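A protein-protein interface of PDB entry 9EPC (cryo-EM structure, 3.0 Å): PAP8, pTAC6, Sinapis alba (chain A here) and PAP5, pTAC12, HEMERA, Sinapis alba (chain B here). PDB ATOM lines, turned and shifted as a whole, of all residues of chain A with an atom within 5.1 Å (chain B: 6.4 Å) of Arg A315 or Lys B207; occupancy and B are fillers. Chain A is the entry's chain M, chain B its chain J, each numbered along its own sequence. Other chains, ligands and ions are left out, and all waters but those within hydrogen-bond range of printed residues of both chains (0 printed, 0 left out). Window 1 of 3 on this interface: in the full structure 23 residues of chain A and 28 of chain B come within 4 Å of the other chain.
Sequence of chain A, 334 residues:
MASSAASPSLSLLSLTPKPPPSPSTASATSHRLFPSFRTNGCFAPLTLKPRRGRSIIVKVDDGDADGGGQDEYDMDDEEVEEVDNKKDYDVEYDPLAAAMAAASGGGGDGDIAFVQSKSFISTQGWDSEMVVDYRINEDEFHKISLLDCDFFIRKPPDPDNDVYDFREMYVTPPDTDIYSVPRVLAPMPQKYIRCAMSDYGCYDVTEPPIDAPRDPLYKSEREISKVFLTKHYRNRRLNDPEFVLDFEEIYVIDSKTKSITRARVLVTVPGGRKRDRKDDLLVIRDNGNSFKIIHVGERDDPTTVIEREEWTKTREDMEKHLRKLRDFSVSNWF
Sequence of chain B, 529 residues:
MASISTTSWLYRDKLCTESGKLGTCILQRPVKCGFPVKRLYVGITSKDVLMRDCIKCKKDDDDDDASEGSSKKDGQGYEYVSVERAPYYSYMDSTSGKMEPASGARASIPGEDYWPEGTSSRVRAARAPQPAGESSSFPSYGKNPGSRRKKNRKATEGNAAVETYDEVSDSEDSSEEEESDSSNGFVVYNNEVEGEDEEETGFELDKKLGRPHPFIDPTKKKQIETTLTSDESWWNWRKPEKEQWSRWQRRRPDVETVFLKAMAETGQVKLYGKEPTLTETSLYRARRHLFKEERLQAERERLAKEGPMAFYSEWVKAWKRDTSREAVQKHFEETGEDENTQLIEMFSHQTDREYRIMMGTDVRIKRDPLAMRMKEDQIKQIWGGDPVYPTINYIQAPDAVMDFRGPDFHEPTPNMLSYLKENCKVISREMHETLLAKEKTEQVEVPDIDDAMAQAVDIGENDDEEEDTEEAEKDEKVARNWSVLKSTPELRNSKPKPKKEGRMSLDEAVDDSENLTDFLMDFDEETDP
Of the 11 printed residues of chain A, 4 touch a printed residue of chain B. Printed residues of chain A that touch a printed residue of chain B: Trp A311, Arg A315, Glu A319 and Trp A333. Hydrophobic or aromatic side chains of chain A within 4 Å of the printed part of chain B: Trp A311 and Trp A333.
Lys B207 touches just these residues of chain A: Arg A315 and Glu A319. Printed residues of chain A within 4 Å of Phe B215: Arg A315 (3.9 Å). Of the printed residues of chain B, Trp A311 touches Gly B210 (3.7 Å).
NH2 of Arg A315 is in hydrogen-bond range of NE2 of His B213 (3.1 Å). OE1 of Glu A319 is in salt-bridge range of NZ of Lys B207, at 3.3 Å. The indole nitrogen (NE1) of Trp A333 is in hydrogen-bond range of the backbone carbonyl oxygen (O) of Gly B210, at 2.8 Å. N of Trp A333 lies within hydrogen-bond range of O of His B213, at 2.6 Å. NH1 of Arg A315 lies close to NZ of Lys B207 (3.1 Å).
Among the printed residues, pairs that only touch across the chains: Trp A311 with Gly B210, Arg A315 with Phe B215 and Trp A333 with Arg B211.
OG1 of Thr A314 sits at hydrogen-bond distance from O of Trp A311 (3.3 Å). The side-chain carboxylate (OE1) of Glu A319 is in salt-bridge range of the guanidinium group (NH1) of Arg A315 (2.5 Å). OD1 of Asp B206 lies within salt-bridge range of NH2 of Arg B211 (2.8 Å).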
ATOM      1  N   GLU A 310     -24.842  18.015 -27.072  1.00  0.00           N
ATOM      2  CA  GLU A 310     -25.724  19.049 -26.541  1.00  0.00           C
ATOM      3  C   GLU A 310     -25.823  18.968 -25.025  1.00  0.00           C
ATOM      4  O   GLU A 310     -25.907  19.999 -24.348  1.00  0.00           O
ATOM      5  CB  GLU A 310     -27.109  18.934 -27.172  1.00  0.00           C
ATOM      6  CG  GLU A 310     -27.147  19.267 -28.648  1.00  0.00           C
ATOM      7  CD  GLU A 310     -28.547  19.201 -29.220  1.00  0.00           C
ATOM      8  OE1 GLU A 310     -29.461  18.744 -28.504  1.00  0.00           O
ATOM      9  OE2 GLU A 310     -28.732  19.609 -30.386  1.00  0.00           O
ATOM     10  N   TRP A 311     -25.833  17.755 -24.475  1.00  0.00           N
ATOM     11  CA  TRP A 311     -25.919  17.608 -23.027  1.00  0.00           C
ATOM     12  C   TRP A 311     -24.681  18.170 -22.343  1.00  0.00           C
ATOM     13  O   TRP A 311     -24.785  18.830 -21.306  1.00  0.00           O
ATOM     14  CB  TRP A 311     -26.119  16.141 -22.659  1.00  0.00           C
ATOM     15  CG  TRP A 311     -26.695  15.942 -21.298  1.00  0.00           C
ATOM     16  CD1 TRP A 311     -28.012  15.788 -20.982  1.00  0.00           C
ATOM     17  CD2 TRP A 311     -25.977  15.879 -20.064  1.00  0.00           C
ATOM     18  NE1 TRP A 311     -28.157  15.630 -19.628  1.00  0.00           N
ATOM     19  CE2 TRP A 311     -26.921  15.681 -19.041  1.00  0.00           C
ATOM     20  CE3 TRP A 311     -24.625  15.967 -19.725  1.00  0.00           C
ATOM     21  CZ2 TRP A 311     -26.559  15.573 -17.705  1.00  0.00           C
ATOM     22  CZ3 TRP A 311     -24.268  15.860 -18.400  1.00  0.00           C
ATOM     23  CH2 TRP A 311     -25.229  15.665 -17.406  1.00  0.00           C
ATOM     24  N   THR A 312     -23.501  17.916 -22.910  1.00  0.00           N
ATOM     25  CA  THR A 312     -22.273  18.440 -22.325  1.00  0.00           C
ATOM     26  C   THR A 312     -22.249  19.962 -22.362  1.00  0.00           C
ATOM     27  O   THR A 312     -21.862  20.609 -21.383  1.00  0.00           O
ATOM     28  CB  THR A 312     -21.061  17.870 -23.059  1.00  0.00           C
ATOM     29  OG1 THR A 312     -21.076  16.441 -22.967  1.00  0.00           O
ATOM     30  CG2 THR A 312     -19.776  18.393 -22.448  1.00  0.00           C
ATOM     31  N   LYS A 313     -22.665  20.552 -23.483  1.00  0.00           N
ATOM     32  CA  LYS A 313     -22.628  22.003 -23.617  1.00  0.00           C
ATOM     33  C   LYS A 313     -23.611  22.674 -22.668  1.00  0.00           C
ATOM     34  O   LYS A 313     -23.254  23.616 -21.952  1.00  0.00           O
ATOM     35  CB  LYS A 313     -22.922  22.400 -25.061  1.00  0.00           C
ATOM     36  CG  LYS A 313     -23.176  23.881 -25.250  1.00  0.00           C
ATOM     37  CD  LYS A 313     -23.555  24.192 -26.686  1.00  0.00           C
ATOM     38  CE  LYS A 313     -23.926  25.655 -26.852  1.00  0.00           C
ATOM     39  NZ  LYS A 313     -25.086  26.027 -25.996  1.00  0.00           N
ATOM     40  N   THR A 314     -24.859  22.204 -22.650  1.00  0.00           N
ATOM     41  CA  THR A 314     -25.871  22.832 -21.810  1.00  0.00           C
ATOM     42  C   THR A 314     -25.581  22.636 -20.329  1.00  0.00           C
ATOM     43  O   THR A 314     -25.892  23.515 -19.519  1.00  0.00           O
ATOM     44  CB  THR A 314     -27.252  22.283 -22.151  1.00  0.00           C
ATOM     45  OG1 THR A 314     -27.221  20.853 -22.088  1.00  0.00           O
ATOM     46  CG2 THR A 314     -27.661  22.715 -23.544  1.00  0.00           C
ATOM     47  N   ARG A 315     -24.998  21.496 -19.955  1.00  0.00           N
ATOM     48  CA  ARG A 315     -24.667  21.266 -18.554  1.00  0.00           C
ATOM     49  C   ARG A 315     -23.660  22.294 -18.059  1.00  0.00           C
ATOM     50  O   ARG A 315     -23.801  22.830 -16.955  1.00  0.00           O
ATOM     51  CB  ARG A 315     -24.129  19.847 -18.371  1.00  0.00           C
ATOM     52  CG  ARG A 315     -24.428  19.220 -17.017  1.00  0.00           C
ATOM     53  CD  ARG A 315     -23.549  19.797 -15.932  1.00  0.00           C
ATOM     54  NE  ARG A 315     -23.895  19.296 -14.611  1.00  0.00           N
ATOM     55  CZ  ARG A 315     -23.342  19.730 -13.487  1.00  0.00           C
ATOM     56  NH1 ARG A 315     -22.427  20.683 -13.492  1.00  0.00           N
ATOM     57  NH2 ARG A 315     -23.718  19.194 -12.330  1.00  0.00           N
ATOM     58  N   GLU A 316     -22.640  22.583 -18.865  1.00  0.00           N
ATOM     59  CA  GLU A 316     -21.660  23.592 -18.483  1.00  0.00           C
ATOM     60  C   GLU A 316     -22.286  24.980 -18.444  1.00  0.00           C
ATOM     61  O   GLU A 316     -21.970  25.785 -17.560  1.00  0.00           O
ATOM     62  CB  GLU A 316     -20.475  23.552 -19.446  1.00  0.00           C
ATOM     63  CG  GLU A 316     -19.259  24.331 -18.983  1.00  0.00           C
ATOM     64  CD  GLU A 316     -19.233  25.751 -19.511  1.00  0.00           C
ATOM     65  OE1 GLU A 316     -20.126  26.109 -20.307  1.00  0.00           O
ATOM     66  OE2 GLU A 316     -18.314  26.508 -19.135  1.00  0.00           O
ATOM     67  N   ASP A 317     -23.173  25.281 -19.394  1.00  0.00           N
ATOM     68  CA  ASP A 317     -23.838  26.580 -19.403  1.00  0.00           C
ATOM     69  C   ASP A 317     -24.769  26.737 -18.209  1.00  0.00           C
ATOM     70  O   ASP A 317     -24.840  27.817 -17.610  1.00  0.00           O
ATOM     71  CB  ASP A 317     -24.611  26.763 -20.707  1.00  0.00           C
ATOM     72  CG  ASP A 317     -23.707  26.805 -21.916  1.00  0.00           C
ATOM     73  OD1 ASP A 317     -22.474  26.739 -21.739  1.00  0.00           O
ATOM     74  OD2 ASP A 317     -24.227  26.903 -23.047  1.00  0.00           O
ATOM     75  N   MET A 318     -25.499  25.679 -17.856  1.00  0.00           N
ATOM     76  CA  MET A 318     -26.397  25.752 -16.709  1.00  0.00           C
ATOM     77  C   MET A 318     -25.624  25.988 -15.420  1.00  0.00           C
ATOM     78  O   MET A 318     -26.055  26.766 -14.563  1.00  0.00           O
ATOM     79  CB  MET A 318     -27.221  24.471 -16.609  1.00  0.00           C
ATOM     80  CG  MET A 318     -28.269  24.476 -15.511  1.00  0.00           C
ATOM     81  SD  MET A 318     -29.833  25.203 -16.028  1.00  0.00           S
ATOM     82  CE  MET A 318     -29.849  26.700 -15.054  1.00  0.00           C
ATOM     83  N   GLU A 319     -24.481  25.319 -15.262  1.00  0.00           N
ATOM     84  CA  GLU A 319     -23.685  25.496 -14.053  1.00  0.00           C
ATOM     85  C   GLU A 319     -23.177  26.925 -13.928  1.00  0.00           C
ATOM     86  O   GLU A 319     -23.207  27.509 -12.840  1.00  0.00           O
ATOM     87  CB  GLU A 319     -22.520  24.510 -14.042  1.00  0.00           C
ATOM     88  CG  GLU A 319     -21.624  24.640 -12.826  1.00  0.00           C
ATOM     89  CD  GLU A 319     -20.555  23.571 -12.775  1.00  0.00           C
ATOM     90  OE1 GLU A 319     -20.729  22.521 -13.429  1.00  0.00           O
ATOM     91  OE2 GLU A 319     -19.536  23.781 -12.085  1.00  0.00           O
ATOM     92  N   TRP A 333     -26.849  18.856  -7.832  1.00  0.00           N
ATOM     93  CA  TRP A 333     -27.258  18.772  -9.223  1.00  0.00           C
ATOM     94  C   TRP A 333     -28.207  17.598  -9.409  1.00  0.00           C
ATOM     95  O   TRP A 333     -28.068  16.561  -8.759  1.00  0.00           O
ATOM     96  CB  TRP A 333     -26.053  18.605 -10.146  1.00  0.00           C
ATOM     97  CG  TRP A 333     -26.404  17.959 -11.447  1.00  0.00           C
ATOM     98  CD1 TRP A 333     -26.294  16.638 -11.763  1.00  0.00           C
ATOM     99  CD2 TRP A 333     -26.938  18.604 -12.607  1.00  0.00           C
ATOM    100  NE1 TRP A 333     -26.723  16.422 -13.047  1.00  0.00           N
ATOM    101  CE2 TRP A 333     -27.120  17.615 -13.587  1.00  0.00           C
ATOM    102  CE3 TRP A 333     -27.274  19.924 -12.910  1.00  0.00           C
ATOM    103  CZ2 TRP A 333     -27.627  17.902 -14.848  1.00  0.00           C
ATOM    104  CZ3 TRP A 333     -27.775  20.206 -14.162  1.00  0.00           C
ATOM    105  CH2 TRP A 333     -27.947  19.202 -15.116  1.00  0.00           C
ATOM    106  N   GLY B 202     -18.030   7.419  -7.302  1.00  0.00           N
ATOM    107  CA  GLY B 202     -18.551   8.503  -6.487  1.00  0.00           C
ATOM    108  C   GLY B 202     -18.635   9.782  -7.291  1.00  0.00           C
ATOM    109  O   GLY B 202     -19.250   9.830  -8.362  1.00  0.00           O
ATOM    110  N   PHE B 203     -18.010  10.836  -6.778  1.00  0.00           N
ATOM    111  CA  PHE B 203     -17.935  12.076  -7.528  1.00  0.00           C
ATOM    112  C   PHE B 203     -17.082  11.871  -8.775  1.00  0.00           C
ATOM    113  O   PHE B 203     -16.293  10.927  -8.868  1.00  0.00           O
ATOM    114  CB  PHE B 203     -17.362  13.197  -6.664  1.00  0.00           C
ATOM    115  CG  PHE B 203     -17.732  14.573  -7.135  1.00  0.00           C
ATOM    116  CD1 PHE B 203     -18.902  15.169  -6.709  1.00  0.00           C
ATOM    117  CD2 PHE B 203     -16.912  15.267  -8.005  1.00  0.00           C
ATOM    118  CE1 PHE B 203     -19.246  16.430  -7.140  1.00  0.00           C
ATOM    119  CE2 PHE B 203     -17.255  16.527  -8.441  1.00  0.00           C
ATOM    120  CZ  PHE B 203     -18.422  17.109  -8.007  1.00  0.00           C
ATOM    121  N   GLU B 204     -17.291  12.750  -9.757  1.00  0.00           N
ATOM    122  CA  GLU B 204     -16.632  12.709 -11.061  1.00  0.00           C
ATOM    123  C   GLU B 204     -17.195  11.564 -11.896  1.00  0.00           C
ATOM    124  O   GLU B 204     -16.879  11.435 -13.081  1.00  0.00           O
ATOM    125  CB  GLU B 204     -15.110  12.594 -10.916  1.00  0.00           C
ATOM    126  CG  GLU B 204     -14.330  12.976 -12.160  1.00  0.00           C
ATOM    127  CD  GLU B 204     -14.552  14.420 -12.564  1.00  0.00           C
ATOM    128  OE1 GLU B 204     -14.733  15.270 -11.667  1.00  0.00           O
ATOM    129  OE2 GLU B 204     -14.551  14.704 -13.780  1.00  0.00           O
ATOM    130  N   LEU B 205     -18.042  10.742 -11.287  1.00  0.00           N
ATOM    131  CA  LEU B 205     -18.846   9.757 -11.996  1.00  0.00           C
ATOM    132  C   LEU B 205     -20.323  10.102 -11.987  1.00  0.00           C
ATOM    133  O   LEU B 205     -20.987   9.981 -13.017  1.00  0.00           O
ATOM    134  CB  LEU B 205     -18.650   8.366 -11.386  1.00  0.00           C
ATOM    135  CG  LEU B 205     -19.484   7.248 -12.012  1.00  0.00           C
ATOM    136  CD1 LEU B 205     -19.164   7.110 -13.488  1.00  0.00           C
ATOM    137  CD2 LEU B 205     -19.252   5.935 -11.288  1.00  0.00           C
ATOM    138  N   ASP B 206     -20.851  10.530 -10.840  1.00  0.00           N
ATOM    139  CA  ASP B 206     -22.188  11.106 -10.818  1.00  0.00           C
ATOM    140  C   ASP B 206     -22.236  12.387 -11.636  1.00  0.00           C
ATOM    141  O   ASP B 206     -23.215  12.647 -12.343  1.00  0.00           O
ATOM    142  CB  ASP B 206     -22.622  11.371  -9.376  1.00  0.00           C
ATOM    143  CG  ASP B 206     -22.650  10.111  -8.537  1.00  0.00           C
ATOM    144  OD1 ASP B 206     -22.926   9.029  -9.095  1.00  0.00           O
ATOM    145  OD2 ASP B 206     -22.397  10.202  -7.318  1.00  0.00           O
ATOM    146  N   LYS B 207     -21.183  13.204 -11.548  1.00  0.00           N
ATOM    147  CA  LYS B 207     -21.117  14.418 -12.353  1.00  0.00           C
ATOM    148  C   LYS B 207     -21.047  14.091 -13.838  1.00  0.00           C
ATOM    149  O   LYS B 207     -21.676  14.767 -14.660  1.00  0.00           O
ATOM    150  CB  LYS B 207     -19.916  15.260 -11.932  1.00  0.00           C
ATOM    151  CG  LYS B 207     -19.808  16.587 -12.657  1.00  0.00           C
ATOM    152  CD  LYS B 207     -18.574  17.351 -12.221  1.00  0.00           C
ATOM    153  CE  LYS B 207     -18.478  18.688 -12.932  1.00  0.00           C
ATOM    154  NZ  LYS B 207     -19.655  19.549 -12.642  1.00  0.00           N
ATOM    155  N   LYS B 208     -20.277  13.065 -14.203  1.00  0.00           N
ATOM    156  CA  LYS B 208     -20.193  12.669 -15.603  1.00  0.00           C
ATOM    157  C   LYS B 208     -21.534  12.166 -16.119  1.00  0.00           C
ATOM    158  O   LYS B 208     -21.953  12.518 -17.227  1.00  0.00           O
ATOM    159  CB  LYS B 208     -19.122  11.596 -15.782  1.00  0.00           C
ATOM    160  CG  LYS B 208     -19.098  10.980 -17.166  1.00  0.00           C
ATOM    161  CD  LYS B 208     -18.305   9.687 -17.182  1.00  0.00           C
ATOM    162  CE  LYS B 208     -18.438   8.974 -18.516  1.00  0.00           C
ATOM    163  NZ  LYS B 208     -17.784   7.638 -18.499  1.00  0.00           N
ATOM    164  N   LEU B 209     -22.224  11.346 -15.331  1.00  0.00           N
ATOM    165  CA  LEU B 209     -23.485  10.756 -15.753  1.00  0.00           C
ATOM    166  C   LEU B 209     -24.694  11.625 -15.441  1.00  0.00           C
ATOM    167  O   LEU B 209     -25.800  11.297 -15.882  1.00  0.00           O
ATOM    168  CB  LEU B 209     -23.671   9.385 -15.100  1.00  0.00           C
ATOM    169  CG  LEU B 209     -22.603   8.352 -15.443  1.00  0.00           C
ATOM    170  CD1 LEU B 209     -22.932   7.015 -14.810  1.00  0.00           C
ATOM    171  CD2 LEU B 209     -22.469   8.218 -16.947  1.00  0.00           C
ATOM    172  N   GLY B 210     -24.519  12.715 -14.703  1.00  0.00           N
ATOM    173  CA  GLY B 210     -25.637  13.559 -14.352  1.00  0.00           C
ATOM    174  C   GLY B 210     -26.444  13.091 -13.164  1.00  0.00           C
ATOM    175  O   GLY B 210     -27.474  13.700 -12.859  1.00  0.00           O
ATOM    176  N   ARG B 211     -26.014  12.030 -12.487  1.00  0.00           N
ATOM    177  CA  ARG B 211     -26.712  11.557 -11.307  1.00  0.00           C
ATOM    178  C   ARG B 211     -26.578  12.577 -10.180  1.00  0.00           C
ATOM    179  O   ARG B 211     -25.642  13.377 -10.169  1.00  0.00           O
ATOM    180  CB  ARG B 211     -26.163  10.201 -10.880  1.00  0.00           C
ATOM    181  CG  ARG B 211     -26.402   9.111 -11.905  1.00  0.00           C
ATOM    182  CD  ARG B 211     -26.045   7.740 -11.369  1.00  0.00           C
ATOM    183  NE  ARG B 211     -24.643   7.654 -10.982  1.00  0.00           N
ATOM    184  CZ  ARG B 211     -24.013   6.520 -10.711  1.00  0.00           C
ATOM    185  NH1 ARG B 211     -24.629   5.352 -10.790  1.00  0.00           N
ATOM    186  NH2 ARG B 211     -22.733   6.558 -10.356  1.00  0.00           N
ATOM    187  N   HIS B 213     -25.594  14.836  -7.362  1.00  0.00           N
ATOM    188  CA  HIS B 213     -24.301  15.048  -6.728  1.00  0.00           C
ATOM    189  C   HIS B 213     -24.194  16.516  -6.354  1.00  0.00           C
ATOM    190  O   HIS B 213     -24.881  17.359  -6.941  1.00  0.00           O
ATOM    191  CB  HIS B 213     -23.153  14.650  -7.665  1.00  0.00           C
ATOM    192  CG  HIS B 213     -22.966  15.588  -8.815  1.00  0.00           C
ATOM    193  ND1 HIS B 213     -22.204  16.732  -8.726  1.00  0.00           N
ATOM    194  CD2 HIS B 213     -23.453  15.558 -10.077  1.00  0.00           C
ATOM    195  CE1 HIS B 213     -22.223  17.362  -9.886  1.00  0.00           C
ATOM    196  NE2 HIS B 213     -22.974  16.671 -10.723  1.00  0.00           N
ATOM    197  N   PRO B 214     -23.352  16.856  -5.382  1.00  0.00           N
ATOM    198  CA  PRO B 214     -23.134  18.270  -5.070  1.00  0.00           C
ATOM    199  C   PRO B 214     -22.486  18.989  -6.242  1.00  0.00           C
ATOM    200  O   PRO B 214     -21.731  18.401  -7.017  1.00  0.00           O
ATOM    201  CB  PRO B 214     -22.205  18.230  -3.854  1.00  0.00           C
ATOM    202  CG  PRO B 214     -22.390  16.874  -3.277  1.00  0.00           C
ATOM    203  CD  PRO B 214     -22.643  15.975  -4.442  1.00  0.00           C
ATOM    204  N   PHE B 215     -22.802  20.277  -6.373  1.00  0.00           N
ATOM    205  CA  PHE B 215     -22.197  21.069  -7.438  1.00  0.00           C
ATOM    206  C   PHE B 215     -20.693  21.193  -7.244  1.00  0.00           C
ATOM    207  O   PHE B 215     -19.929  21.170  -8.215  1.00  0.00           O
ATOM    208  CB  PHE B 215     -22.842  22.450  -7.500  1.00  0.00           C
ATOM    209  CG  PHE B 215     -24.030  22.519  -8.405  1.00  0.00           C
ATOM    210  CD1 PHE B 215     -23.881  22.385  -9.771  1.00  0.00           C
ATOM    211  CD2 PHE B 215     -25.294  22.731  -7.891  1.00  0.00           C
ATOM    212  CE1 PHE B 215     -24.973  22.454 -10.608  1.00  0.00           C
ATOM    213  CE2 PHE B 215     -26.388  22.801  -8.723  1.00  0.00           C
ATOM    214  CZ  PHE B 215     -26.229  22.662 -10.082  1.00  0.00           C
